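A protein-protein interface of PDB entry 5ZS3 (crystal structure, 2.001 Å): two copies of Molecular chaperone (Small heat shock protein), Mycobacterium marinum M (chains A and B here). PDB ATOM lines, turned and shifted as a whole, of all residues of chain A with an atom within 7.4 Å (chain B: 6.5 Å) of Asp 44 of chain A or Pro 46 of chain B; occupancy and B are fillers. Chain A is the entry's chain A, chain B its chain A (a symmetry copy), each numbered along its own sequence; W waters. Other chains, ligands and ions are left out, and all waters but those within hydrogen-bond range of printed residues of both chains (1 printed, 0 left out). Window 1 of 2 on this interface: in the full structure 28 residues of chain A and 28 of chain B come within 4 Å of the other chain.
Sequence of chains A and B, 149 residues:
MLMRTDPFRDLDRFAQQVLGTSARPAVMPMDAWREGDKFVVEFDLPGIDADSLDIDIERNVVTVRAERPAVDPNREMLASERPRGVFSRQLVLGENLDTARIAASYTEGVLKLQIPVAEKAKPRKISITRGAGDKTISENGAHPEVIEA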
ATOM      1  N   VAL A  27      25.219  -0.138   5.032  1.00  0.00           N
ATOM      2  CA  VAL A  27      23.809   0.161   4.846  1.00  0.00           C
ATOM      3  C   VAL A  27      23.035  -0.372   6.043  1.00  0.00           C
ATOM      4  O   VAL A  27      23.436  -1.349   6.690  1.00  0.00           O
ATOM      5  CB  VAL A  27      23.322  -0.444   3.508  1.00  0.00           C
ATOM      6  CG1 VAL A  27      23.241  -1.958   3.614  1.00  0.00           C
ATOM      7  CG2 VAL A  27      21.975   0.140   3.106  1.00  0.00           C
ATOM      8  N   MET A  28      21.944   0.299   6.372  1.00  0.00           N
ATOM      9  CA  MET A  28      21.148  -0.190   7.479  1.00  0.00           C
ATOM     10  C   MET A  28      19.744  -0.449   6.989  1.00  0.00           C
ATOM     11  O   MET A  28      19.216   0.304   6.153  1.00  0.00           O
ATOM     12  CB  MET A  28      21.153   0.780   8.663  1.00  0.00           C
ATOM     13  CG  MET A  28      20.567   2.118   8.377  1.00  0.00           C
ATOM     14  SD  MET A  28      21.815   3.199   7.435  1.00  0.00           S
ATOM     15  CE  MET A  28      20.966   4.874   8.033  1.00  0.00           C
ATOM     16  N   PRO A  29      19.128  -1.500   7.516  1.00  0.00           N
ATOM     17  CA  PRO A  29      17.811  -1.886   7.015  1.00  0.00           C
ATOM     18  C   PRO A  29      16.753  -0.890   7.449  1.00  0.00           C
ATOM     19  O   PRO A  29      16.843  -0.263   8.515  1.00  0.00           O
ATOM     20  CB  PRO A  29      17.592  -3.279   7.633  1.00  0.00           C
ATOM     21  CG  PRO A  29      18.371  -3.257   8.887  1.00  0.00           C
ATOM     22  CD  PRO A  29      19.579  -2.373   8.628  1.00  0.00           C
ATOM     23  N   MET A  30      15.713  -0.805   6.621  1.00  0.00           N
ATOM     24  CA  MET A  30      14.705   0.224   6.704  1.00  0.00           C
ATOM     25  C   MET A  30      13.292  -0.361   6.611  1.00  0.00           C
ATOM     26  O   MET A  30      13.060  -1.213   5.751  1.00  0.00           O
ATOM     27  CB  MET A  30      14.931   1.185   5.539  1.00  0.00           C
ATOM     28  CG  MET A  30      13.797   2.102   5.207  1.00  0.00           C
ATOM     29  SD  MET A  30      14.340   3.385   3.882  1.00  0.00           S
ATOM     30  CE  MET A  30      14.147   2.385   2.098  1.00  0.00           C
ATOM     31  N   ASP A  31      12.362   0.083   7.455  1.00  0.00           N
ATOM     32  CA  ASP A  31      10.938  -0.091   7.201  1.00  0.00           C
ATOM     33  C   ASP A  31      10.357   1.283   6.908  1.00  0.00           C
ATOM     34  O   ASP A  31      10.715   2.253   7.572  1.00  0.00           O
ATOM     35  CB  ASP A  31      10.198  -0.676   8.412  1.00  0.00           C
ATOM     36  CG  ASP A  31      10.585  -2.129   8.740  1.00  0.00           C
ATOM     37  OD1 ASP A  31      11.075  -2.881   7.874  1.00  0.00           O
ATOM     38  OD2 ASP A  31      10.358  -2.512   9.922  1.00  0.00           O
ATOM     39  N   GLU A  42      11.761   3.813   9.665  1.00  0.00           N
ATOM     40  CA  GLU A  42      12.548   3.371  10.813  1.00  0.00           C
ATOM     41  C   GLU A  42      13.796   2.632  10.355  1.00  0.00           C
ATOM     42  O   GLU A  42      13.741   1.843   9.411  1.00  0.00           O
ATOM     43  CB  GLU A  42      11.733   2.457  11.734  1.00  0.00           C
ATOM     44  CG  GLU A  42      10.790   3.214  12.643  1.00  0.00           C
ATOM     45  CD  GLU A  42       9.990   2.280  13.570  1.00  0.00           C
ATOM     46  OE1 GLU A  42       9.888   1.059  13.280  1.00  0.00           O
ATOM     47  OE2 GLU A  42       9.460   2.776  14.587  1.00  0.00           O
ATOM     48  N   PHE A  43      14.926   2.924  10.995  1.00  0.00           N
ATOM     49  CA  PHE A  43      16.198   2.298  10.662  1.00  0.00           C
ATOM     50  C   PHE A  43      16.698   1.523  11.868  1.00  0.00           C
ATOM     51  O   PHE A  43      16.654   2.036  12.989  1.00  0.00           O
ATOM     52  CB  PHE A  43      17.273   3.328  10.280  1.00  0.00           C
ATOM     53  CG  PHE A  43      16.929   4.170   9.092  1.00  0.00           C
ATOM     54  CD1 PHE A  43      17.203   3.736   7.806  1.00  0.00           C
ATOM     55  CD2 PHE A  43      16.328   5.406   9.267  1.00  0.00           C
ATOM     56  CE1 PHE A  43      16.902   4.543   6.711  1.00  0.00           C
ATOM     57  CE2 PHE A  43      16.002   6.210   8.184  1.00  0.00           C
ATOM     58  CZ  PHE A  43      16.298   5.786   6.905  1.00  0.00           C
ATOM     59  N   ASP A  44      17.195   0.304  11.647  1.00  0.00           N
ATOM     60  CA  ASP A  44      17.953  -0.397  12.687  1.00  0.00           C
ATOM     61  C   ASP A  44      19.358   0.189  12.720  1.00  0.00           C
ATOM     62  O   ASP A  44      20.138  -0.005  11.784  1.00  0.00           O
ATOM     63  CB  ASP A  44      18.034  -1.899  12.436  1.00  0.00           C
ATOM     64  CG  ASP A  44      16.734  -2.643  12.712  1.00  0.00           C
ATOM     65  OD1 ASP A  44      15.834  -2.125  13.419  1.00  0.00           O
ATOM     66  OD2 ASP A  44      16.618  -3.768  12.168  1.00  0.00           O
ATOM     67  N   LEU A  45      19.682   0.910  13.788  1.00  0.00           N
ATOM     68  CA  LEU A  45      20.989   1.555  13.940  1.00  0.00           C
ATOM     69  C   LEU A  45      21.494   1.351  15.360  1.00  0.00           C
ATOM     70  O   LEU A  45      21.737   2.312  16.094  1.00  0.00           O
ATOM     71  CB  LEU A  45      20.883   3.044  13.614  1.00  0.00           C
ATOM     72  CG  LEU A  45      21.056   3.449  12.160  1.00  0.00           C
ATOM     73  CD1 LEU A  45      20.908   4.974  12.056  1.00  0.00           C
ATOM     74  CD2 LEU A  45      22.432   2.992  11.679  1.00  0.00           C
ATOM     75  N   PRO A  46      21.656   0.100  15.786  1.00  0.00           N
ATOM     76  CA  PRO A  46      21.987  -0.155  17.192  1.00  0.00           C
ATOM     77  C   PRO A  46      23.359   0.371  17.551  1.00  0.00           C
ATOM     78  O   PRO A  46      24.278   0.370  16.731  1.00  0.00           O
ATOM     79  CB  PRO A  46      21.948  -1.684  17.301  1.00  0.00           C
ATOM     80  CG  PRO A  46      22.265  -2.162  15.938  1.00  0.00           C
ATOM     81  CD  PRO A  46      21.687  -1.129  14.974  1.00  0.00           C
ATOM     82  N   GLY A  47      23.484   0.828  18.795  1.00  0.00           N
ATOM     83  CA  GLY A  47      24.792   1.087  19.367  1.00  0.00           C
ATOM     84  C   GLY A  47      25.492   2.299  18.802  1.00  0.00           C
ATOM     85  O   GLY A  47      26.724   2.358  18.808  1.00  0.00           O
ATOM     86  N   ILE A  48      24.729   3.291  18.358  1.00  0.00           N
ATOM     87  CA  ILE A  48      25.249   4.541  17.816  1.00  0.00           C
ATOM     88  C   ILE A  48      25.213   5.583  18.922  1.00  0.00           C
ATOM     89  O   ILE A  48      24.197   5.717  19.619  1.00  0.00           O
ATOM     90  CB  ILE A  48      24.410   5.005  16.608  1.00  0.00           C
ATOM     91  CG1 ILE A  48      24.452   3.966  15.493  1.00  0.00           C
ATOM     92  CG2 ILE A  48      24.849   6.373  16.115  1.00  0.00           C
ATOM     93  CD1 ILE A  48      25.794   3.833  14.865  1.00  0.00           C
ATOM     94  N   PHE A  87      27.786   4.514   8.375  1.00  0.00           N
ATOM     95  CA  PHE A  87      26.515   4.083   7.813  1.00  0.00           C
ATOM     96  C   PHE A  87      25.864   5.263   7.114  1.00  0.00           C
ATOM     97  O   PHE A  87      25.933   6.393   7.604  1.00  0.00           O
ATOM     98  CB  PHE A  87      25.567   3.574   8.895  1.00  0.00           C
ATOM     99  CG  PHE A  87      26.070   2.375   9.628  1.00  0.00           C
ATOM    100  CD1 PHE A  87      27.085   2.499  10.558  1.00  0.00           C
ATOM    101  CD2 PHE A  87      25.497   1.132   9.420  1.00  0.00           C
ATOM    102  CE1 PHE A  87      27.557   1.395  11.233  1.00  0.00           C
ATOM    103  CE2 PHE A  87      25.947   0.029  10.107  1.00  0.00           C
ATOM    104  CZ  PHE A  87      26.980   0.162  11.016  1.00  0.00           C
ATOM    105  N   TYR A 106      15.471   8.653  18.298  1.00  0.00           N
ATOM    106  CA  TYR A 106      16.384   7.527  18.358  1.00  0.00           C
ATOM    107  C   TYR A 106      16.185   6.837  19.693  1.00  0.00           C
ATOM    108  O   TYR A 106      16.521   7.393  20.742  1.00  0.00           O
ATOM    109  CB  TYR A 106      17.821   7.995  18.200  1.00  0.00           C
ATOM    110  CG  TYR A 106      18.802   6.864  18.205  1.00  0.00           C
ATOM    111  CD1 TYR A 106      18.799   5.914  17.190  1.00  0.00           C
ATOM    112  CD2 TYR A 106      19.726   6.724  19.236  1.00  0.00           C
ATOM    113  CE1 TYR A 106      19.715   4.856  17.189  1.00  0.00           C
ATOM    114  CE2 TYR A 106      20.632   5.670  19.250  1.00  0.00           C
ATOM    115  CZ  TYR A 106      20.627   4.747  18.224  1.00  0.00           C
ATOM    116  OH  TYR A 106      21.522   3.713  18.241  1.00  0.00           O
ATOM    117  N   THR A 107      15.658   5.623  19.658  1.00  0.00           N
ATOM    118  CA  THR A 107      15.451   4.905  20.894  1.00  0.00           C
ATOM    119  C   THR A 107      15.525   3.411  20.633  1.00  0.00           C
ATOM    120  O   THR A 107      15.100   2.931  19.580  1.00  0.00           O
ATOM    121  CB  THR A 107      14.110   5.283  21.538  1.00  0.00           C
ATOM    122  OG1 THR A 107      13.834   4.394  22.624  1.00  0.00           O
ATOM    123  CG2 THR A 107      12.988   5.182  20.548  1.00  0.00           C
ATOM    124  N   GLU A 108      16.063   2.677  21.603  1.00  0.00           N
ATOM    125  CA  GLU A 108      16.192   1.230  21.491  1.00  0.00           C
ATOM    126  C   GLU A 108      16.973   0.833  20.244  1.00  0.00           C
ATOM    127  O   GLU A 108      16.738  -0.229  19.667  1.00  0.00           O
ATOM    128  CB  GLU A 108      14.813   0.568  21.480  1.00  0.00           C
ATOM    129  CG  GLU A 108      13.979   0.852  22.718  1.00  0.00           C
ATOM    130  CD  GLU A 108      13.656  -0.404  23.504  1.00  0.00           C
ATOM    131  OE1 GLU A 108      13.495  -0.310  24.739  1.00  0.00           O
ATOM    132  OE2 GLU A 108      13.565  -1.486  22.887  1.00  0.00           O
ATOM    133  N   GLY A 109      17.903   1.688  19.832  1.00  0.00           N
ATOM    134  CA  GLY A 109      18.708   1.415  18.661  1.00  0.00           C
ATOM    135  C   GLY A 109      17.978   1.578  17.349  1.00  0.00           C
ATOM    136  O   GLY A 109      18.491   1.147  16.318  1.00  0.00           O
ATOM    137  N   VAL A 110      16.802   2.199  17.350  1.00  0.00           N
ATOM    138  CA  VAL A 110      16.021   2.438  16.133  1.00  0.00           C
ATOM    139  C   VAL A 110      15.933   3.938  15.884  1.00  0.00           C
ATOM    140  O   VAL A 110      15.461   4.691  16.746  1.00  0.00           O
ATOM    141  CB  VAL A 110      14.626   1.811  16.228  1.00  0.00           C
ATOM    142  CG1 VAL A 110      13.858   2.062  14.958  1.00  0.00           C
ATOM    143  CG2 VAL A 110      14.763   0.318  16.489  1.00  0.00           C
ATOM    144  N   LEU A 111      16.378   4.377  14.710  1.00  0.00           N
ATOM    145  CA  LEU A 111      16.180   5.758  14.283  1.00  0.00           C
ATOM    146  C   LEU A 111      14.862   5.861  13.523  1.00  0.00           C
ATOM    147  O   LEU A 111      14.696   5.238  12.473  1.00  0.00           O
ATOM    148  CB  LEU A 111      17.340   6.224  13.416  1.00  0.00           C
ATOM    149  CG  LEU A 111      17.009   7.549  12.757  1.00  0.00           C
ATOM    150  CD1 LEU A 111      16.951   8.625  13.815  1.00  0.00           C
ATOM    151  CD2 LEU A 111      18.066   7.821  11.741  1.00  0.00           C
ATOM    152  N   PHE B  43      25.297  -8.172  21.496  1.00  0.00           N
ATOM    153  CA  PHE B  43      24.480  -8.526  20.342  1.00  0.00           C
ATOM    154  C   PHE B  43      23.763  -7.283  19.844  1.00  0.00           C
ATOM    155  O   PHE B  43      23.217  -6.525  20.650  1.00  0.00           O
ATOM    156  CB  PHE B  43      23.417  -9.583  20.684  1.00  0.00           C
ATOM    157  CG  PHE B  43      23.972 -10.880  21.182  1.00  0.00           C
ATOM    158  CD1 PHE B  43      24.362 -11.875  20.302  1.00  0.00           C
ATOM    159  CD2 PHE B  43      24.103 -11.101  22.544  1.00  0.00           C
ATOM    160  CE1 PHE B  43      24.852 -13.088  20.782  1.00  0.00           C
ATOM    161  CE2 PHE B  43      24.610 -12.296  23.035  1.00  0.00           C
ATOM    162  CZ  PHE B  43      24.976 -13.295  22.157  1.00  0.00           C
ATOM    163  N   ASP B  44      23.738  -7.081  18.526  1.00  0.00           N
ATOM    164  CA  ASP B  44      22.841  -6.082  17.937  1.00  0.00           C
ATOM    165  C   ASP B  44      21.441  -6.678  17.890  1.00  0.00           C
ATOM    166  O   ASP B  44      21.183  -7.608  17.121  1.00  0.00           O
ATOM    167  CB  ASP B  44      23.268  -5.674  16.531  1.00  0.00           C
ATOM    168  CG  ASP B  44      24.495  -4.771  16.495  1.00  0.00           C
ATOM    169  OD1 ASP B  44      24.864  -4.146  17.520  1.00  0.00           O
ATOM    170  OD2 ASP B  44      25.112  -4.725  15.403  1.00  0.00           O
ATOM    171  N   LEU B  45      20.538  -6.152  18.710  1.00  0.00           N
ATOM    172  CA  LEU B  45      19.160  -6.645  18.790  1.00  0.00           C
ATOM    173  C   LEU B  45      18.202  -5.465  18.848  1.00  0.00           C
ATOM    174  O   LEU B  45      17.440  -5.308  19.807  1.00  0.00           O
ATOM    175  CB  LEU B  45      18.990  -7.538  20.018  1.00  0.00           C
ATOM    176  CG  LEU B  45      19.314  -9.013  19.850  1.00  0.00           C
ATOM    177  CD1 LEU B  45      19.082  -9.720  21.193  1.00  0.00           C
ATOM    178  CD2 LEU B  45      18.420  -9.595  18.756  1.00  0.00           C
ATOM    179  N   PRO B  46      18.220  -4.601  17.835  1.00  0.00           N
ATOM    180  CA  PRO B  46      17.433  -3.365  17.915  1.00  0.00           C
ATOM    181  C   PRO B  46      15.948  -3.645  17.930  1.00  0.00           C
ATOM    182  O   PRO B  46      15.470  -4.594  17.308  1.00  0.00           O
ATOM    183  CB  PRO B  46      17.828  -2.603  16.645  1.00  0.00           C
ATOM    184  CG  PRO B  46      18.223  -3.657  15.686  1.00  0.00           C
ATOM    185  CD  PRO B  46      18.843  -4.781  16.512  1.00  0.00           C
ATOM    186  N   GLY B  47      15.218  -2.801  18.657  1.00  0.00           N
ATOM    187  CA  GLY B  47      13.773  -2.765  18.533  1.00  0.00           C
ATOM    188  C   GLY B  47      13.065  -3.959  19.124  1.00  0.00           C
ATOM    189  O   GLY B  47      11.966  -4.305  18.682  1.00  0.00           O
ATOM    190  N   ILE B  48      13.650  -4.568  20.148  1.00  0.00           N
ATOM    191  CA  ILE B  48      13.081  -5.711  20.852  1.00  0.00           C
ATOM    192  C   ILE B  48      12.393  -5.195  22.107  1.00  0.00           C
ATOM    193  O   ILE B  48      12.969  -4.383  22.843  1.00  0.00           O
ATOM    194  CB  ILE B  48      14.178  -6.731  21.217  1.00  0.00           C
ATOM    195  CG1 ILE B  48      14.862  -7.258  19.961  1.00  0.00           C
ATOM    196  CG2 ILE B  48      13.628  -7.862  22.070  1.00  0.00           C
ATOM    197  CD1 ILE B  48      13.973  -8.098  19.115  1.00  0.00           C
ATOM    198  N   ARG B  68      10.877 -10.234  17.539  1.00  0.00           N
ATOM    199  CA  ARG B  68      10.344  -9.009  17.001  1.00  0.00           C
ATOM    200  C   ARG B  68       9.083  -9.369  16.234  1.00  0.00           C
ATOM    201  O   ARG B  68       9.147 -10.172  15.285  1.00  0.00           O
ATOM    202  CB  ARG B  68      11.365  -8.320  16.100  1.00  0.00           C
ATOM    203  CG  ARG B  68      11.050  -6.868  15.827  1.00  0.00           C
ATOM    204  CD  ARG B  68      12.280  -6.002  15.670  1.00  0.00           C
ATOM    205  NE  ARG B  68      13.033  -6.298  14.464  1.00  0.00           N
ATOM    206  CZ  ARG B  68      13.968  -5.490  13.965  1.00  0.00           C
ATOM    207  NH1 ARG B  68      14.248  -4.345  14.585  1.00  0.00           N
ATOM    208  NH2 ARG B  68      14.640  -5.828  12.879  1.00  0.00           N
ATOM    209  N   GLU B  81      12.477  -4.056   5.223  1.00  0.00           N
ATOM    210  CA  GLU B  81      13.751  -4.753   5.154  1.00  0.00           C
ATOM    211  C   GLU B  81      14.204  -5.276   6.500  1.00  0.00           C
ATOM    212  O   GLU B  81      15.098  -6.126   6.541  1.00  0.00           O
ATOM    213  CB  GLU B  81      14.864  -3.831   4.643  1.00  0.00           C
ATOM    214  CG  GLU B  81      14.492  -3.033   3.409  1.00  0.00           C
ATOM    215  CD  GLU B  81      15.567  -1.991   3.072  1.00  0.00           C
ATOM    216  OE1 GLU B  81      16.325  -1.546   3.960  1.00  0.00           O
ATOM    217  OE2 GLU B  81      15.550  -1.535   1.901  1.00  0.00           O
ATOM    218  N   ARG B  82      13.665  -4.753   7.592  1.00  0.00           N
ATOM    219  CA  ARG B  82      14.204  -5.100   8.893  1.00  0.00           C
ATOM    220  C   ARG B  82      13.810  -6.535   9.245  1.00  0.00           C
ATOM    221  O   ARG B  82      12.676  -6.951   8.994  1.00  0.00           O
ATOM    222  CB  ARG B  82      13.713  -4.107   9.948  1.00  0.00           C
ATOM    223  CG  ARG B  82      14.280  -2.710   9.698  1.00  0.00           C
ATOM    224  CD  ARG B  82      13.461  -1.601  10.296  1.00  0.00           C
ATOM    225  NE  ARG B  82      13.614  -1.507  11.739  1.00  0.00           N
ATOM    226  CZ  ARG B  82      12.619  -1.252  12.578  1.00  0.00           C
ATOM    227  NH1 ARG B  82      11.388  -1.076  12.124  1.00  0.00           N
ATOM    228  NH2 ARG B  82      12.862  -1.194  13.875  1.00  0.00           N
ATOM    229  N   PRO B  83      14.741  -7.331   9.764  1.00  0.00           N
ATOM    230  CA  PRO B  83      14.424  -8.729  10.072  1.00  0.00           C
ATOM    231  C   PRO B  83      13.436  -8.826  11.221  1.00  0.00           C
ATOM    232  O   PRO B  83      13.519  -8.080  12.198  1.00  0.00           O
ATOM    233  CB  PRO B  83      15.792  -9.324  10.445  1.00  0.00           C
ATOM    234  CG  PRO B  83      16.615  -8.127  10.893  1.00  0.00           C
ATOM    235  CD  PRO B  83      16.149  -6.992  10.026  1.00  0.00           C
ATOM    236  N   PHE B  87      14.646 -14.518  16.908  1.00  0.00           N
ATOM    237  CA  PHE B  87      16.099 -14.481  16.871  1.00  0.00           C
ATOM    238  C   PHE B  87      16.639 -15.420  17.936  1.00  0.00           C
ATOM    239  O   PHE B  87      16.083 -15.502  19.034  1.00  0.00           O
ATOM    240  CB  PHE B  87      16.632 -13.077  17.145  1.00  0.00           C
ATOM    241  CG  PHE B  87      16.214 -12.062  16.135  1.00  0.00           C
ATOM    242  CD1 PHE B  87      14.919 -11.581  16.121  1.00  0.00           C
ATOM    243  CD2 PHE B  87      17.129 -11.555  15.227  1.00  0.00           C
ATOM    244  CE1 PHE B  87      14.526 -10.648  15.188  1.00  0.00           C
ATOM    245  CE2 PHE B  87      16.751 -10.606  14.307  1.00  0.00           C
ATOM    246  CZ  PHE B  87      15.445 -10.152  14.287  1.00  0.00           C
ATOM    247  N   TYR B 106      20.377  -4.480  28.468  1.00  0.00           N
ATOM    248  CA  TYR B 106      19.850  -4.185  27.148  1.00  0.00           C
ATOM    249  C   TYR B 106      19.672  -2.683  27.044  1.00  0.00           C
ATOM    250  O   TYR B 106      18.809  -2.106  27.712  1.00  0.00           O
ATOM    251  CB  TYR B 106      18.529  -4.903  26.928  1.00  0.00           C
ATOM    252  CG  TYR B 106      17.965  -4.670  25.561  1.00  0.00           C
ATOM    253  CD1 TYR B 106      18.626  -5.136  24.429  1.00  0.00           C
ATOM    254  CD2 TYR B 106      16.779  -3.965  25.387  1.00  0.00           C
ATOM    255  CE1 TYR B 106      18.102  -4.925  23.149  1.00  0.00           C
ATOM    256  CE2 TYR B 106      16.257  -3.738  24.118  1.00  0.00           C
ATOM    257  CZ  TYR B 106      16.917  -4.226  23.008  1.00  0.00           C
ATOM    258  OH  TYR B 106      16.398  -4.002  21.763  1.00  0.00           O
ATOM    259  N   GLU B 108      20.114   0.788  24.091  1.00  0.00           N
ATOM    260  CA  GLU B 108      20.428   1.281  22.755  1.00  0.00           C
ATOM    261  C   GLU B 108      20.347   0.169  21.716  1.00  0.00           C
ATOM    262  O   GLU B 108      21.066   0.191  20.717  1.00  0.00           O
ATOM    263  CB  GLU B 108      21.817   1.921  22.734  1.00  0.00           C
ATOM    264  CG  GLU B 108      21.978   3.088  23.693  1.00  0.00           C
ATOM    265  CD  GLU B 108      22.278   4.392  22.981  1.00  0.00           C
ATOM    266  OE1 GLU B 108      21.899   5.460  23.507  1.00  0.00           O
ATOM    267  OE2 GLU B 108      22.891   4.349  21.894  1.00  0.00           O
ATOM    268  N   GLY B 109      19.470  -0.800  21.954  1.00  0.00           N
ATOM    269  CA  GLY B 109      19.306  -1.906  21.036  1.00  0.00           C
ATOM    270  C   GLY B 109      20.429  -2.916  21.066  1.00  0.00           C
ATOM    271  O   GLY B 109      20.506  -3.756  20.171  1.00  0.00           O
ATOM    272  N   VAL B 110      21.296  -2.871  22.074  1.00  0.00           N
ATOM    273  CA  VAL B 110      22.405  -3.818  22.218  1.00  0.00           C
ATOM    274  C   VAL B 110      22.186  -4.654  23.471  1.00  0.00           C
ATOM    275  O   VAL B 110      22.056  -4.111  24.575  1.00  0.00           O
ATOM    276  CB  VAL B 110      23.757  -3.096  22.265  1.00  0.00           C
ATOM    277  CG1 VAL B 110      24.874  -4.098  22.399  1.00  0.00           C
ATOM    278  CG2 VAL B 110      23.927  -2.266  21.002  1.00  0.00           C
HETATM  279  O   HOH W   1      10.350  -5.401   8.538  1.00  0.00           O
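The backbone NH (N) of Met 30 of chain A lies within hydrogen-bond range of the side-chain carboxylate (OE1) of Glu 81 of chain B, 2.8 Å away.
N of Glu 81 of chain B lies within hydrogen-bond range of OD1 of Asp 31 of chain A (3.2 Å).
The side-chain carboxylate of Asp 31 of chain A is in salt-bridge range of the guanidinium group of Arg 82 of chain B (2.8 Å).
The guanidinium group (NH1) of Arg 82 of chain B lies within salt-bridge range of the side-chain carboxylate (OE1) of Glu 42 of chain A (2.9 Å).
The guanidinium group (NH2) of Arg 68 of chain B is in salt-bridge range of the side-chain carboxylate (OD2) of Asp 44 of chain A, 2.9 Å away.
The side-chain carboxylate of Asp 44 of chain A is in salt-bridge range of the guanidinium group of Arg 82 of chain B (2.9 Å).
O of Glu 108 of chain B sits at hydrogen-bond distance from N of Gly 47 of chain A (3.2 Å).
The backbone carbonyl oxygen of Glu 108 of chain A sits at hydrogen-bond distance from the backbone NH of Gly 47 of chain B, 3.2 Å away.
The side-chain carboxylate (OE2) of Glu 108 of chain B lies close to the backbone carbonyl oxygen (O) of Ile 48 of chain A (3.0 Å).
The backbone carbonyl oxygen (O) of Ile 48 of chain B sits close to the side-chain carboxylate (OE2) of Glu 108 of chain A (3.0 Å).
The backbone carbonyl oxygen of Asp 31 of chain A is in hydrogen-bond range of the backbone NH of Glu 42 of chain A (2.8 Å).
O of Leu 45 of chain A sits at hydrogen-bond distance from OH of Tyr 106 of chain A (2.6 Å).
O of Gly 109 of chain B lies within hydrogen-bond range of N of Leu 45 of chain B (2.8 Å).
O of Pro 46 of chain B sits at hydrogen-bond distance from NH1 of Arg 68 of chain B (3.0 Å).
The backbone NH (N) of Ile 48 of chain B sits at hydrogen-bond distance from the side-chain hydroxyl (OH) of Tyr 106 of chain B.
The backbone carbonyl oxygen (O) of Pro 83 of chain B is in hydrogen-bond range of the guanidinium group (NH2) of Arg 68 of chain B (2.6 Å).
Arg 82 of chain B touches Met 30 of chain A (CD to C, 3.9 Å).
Asp 44 of chain A touches Pro 46 of chain B (CG to CG, 3.5 Å).
OD2 of Asp 44 of chain A touches CD of Pro 83 of chain B, at 3.9 Å.
Pro 46 of chain A touches Glu 108 of chain B.
Pro 46 of chain A touches Gly 109 of chain B.
Val 110 of chain B touches Gly 47 of chain A.
Glu 108 of chain A touches Pro 46 of chain B (O to CA, 3.7 Å).
Gly 109 of chain A touches Pro 46 of chain B.
N of Gly 109 of chain A touches N of Gly 109 of chain B, at 3.6 Å.
N of Gly 47 of chain B touches CG2 of Val 110 of chain A, 3.8 Å away.
Of chain B, only Pro 46, Arg 68, Arg 82 and Pro 83 come within 4 Å of Asp 44 of chain A.
Pro 46 of chain B touches just these residues of chain A: Asp 44 (3.5 Å), Glu 108 (3.7 Å) and Gly 109 (3.8 Å).
Of the printed residues of chain A, Pro 83 of chain B touches Asp 44 (3.9 Å).
Of the printed residues of chain A, Arg 68 of chain B touches Asp 44 (2.9 Å).
Printed residues of chain A within 4 Å of Arg 82 of chain B: Pro 29 (3.7 Å), Met 30 (3.9 Å), Asp 31 (2.8 Å), Glu 42 (2.9 Å), Asp 44 (2.9 Å) and Val 110 (3.6 Å).
Printed residues of chain B within 4 Å of Glu 42 of chain A: Arg 82.
Of the printed residues of chain A, Glu 81 of chain B touches Pro 29 (3.4 Å), Met 30 (2.8 Å) and Asp 31 (3.2 Å).
Thr 107 of chain A touches none of the printed residues of chain B.
Phe 43 of chain A touches none of the printed residues of chain B.
The nearest residue of chain A that does not touch Pro 46 of chain B is Val 110 of chain A (4.2 Å).
The nearest printed residue of chain B that does not touch Ile 48 of chain A is Val 110 of chain B (6.2 Å).
Printed residues of chain B that touch a printed residue of chain A: Asp 44, Pro 46, Gly 47, Ile 48, Arg 68, Glu 81, Arg 82, Pro 83, Tyr 106, Glu 108, Gly 109 and Val 110.
Hydrophobic or aromatic side chains of chain B that line the printed part of chain A: Pro 46, Pro 83, Tyr 106 and Val 110.
Pro 46 of chain A touches Glu 108 of chain B, and with the chains exchanged Glu 108 of chain A touches Pro 46 of chain B.
Pro 46 of chain A touches Gly 109 of chain B, and with the chains exchanged Gly 109 of chain A touches Pro 46 of chain B.
Glu 108 of chain A touches its own counterpart, Glu 108 of chain B.
Gly 109 of chain A touches its own counterpart, Gly 109 of chain B.
Water W1 bridges the side-chain carboxylate (OD1) of Asp 31 of chain A and the backbone carbonyl oxygen (O) of Arg 82 of chain B.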
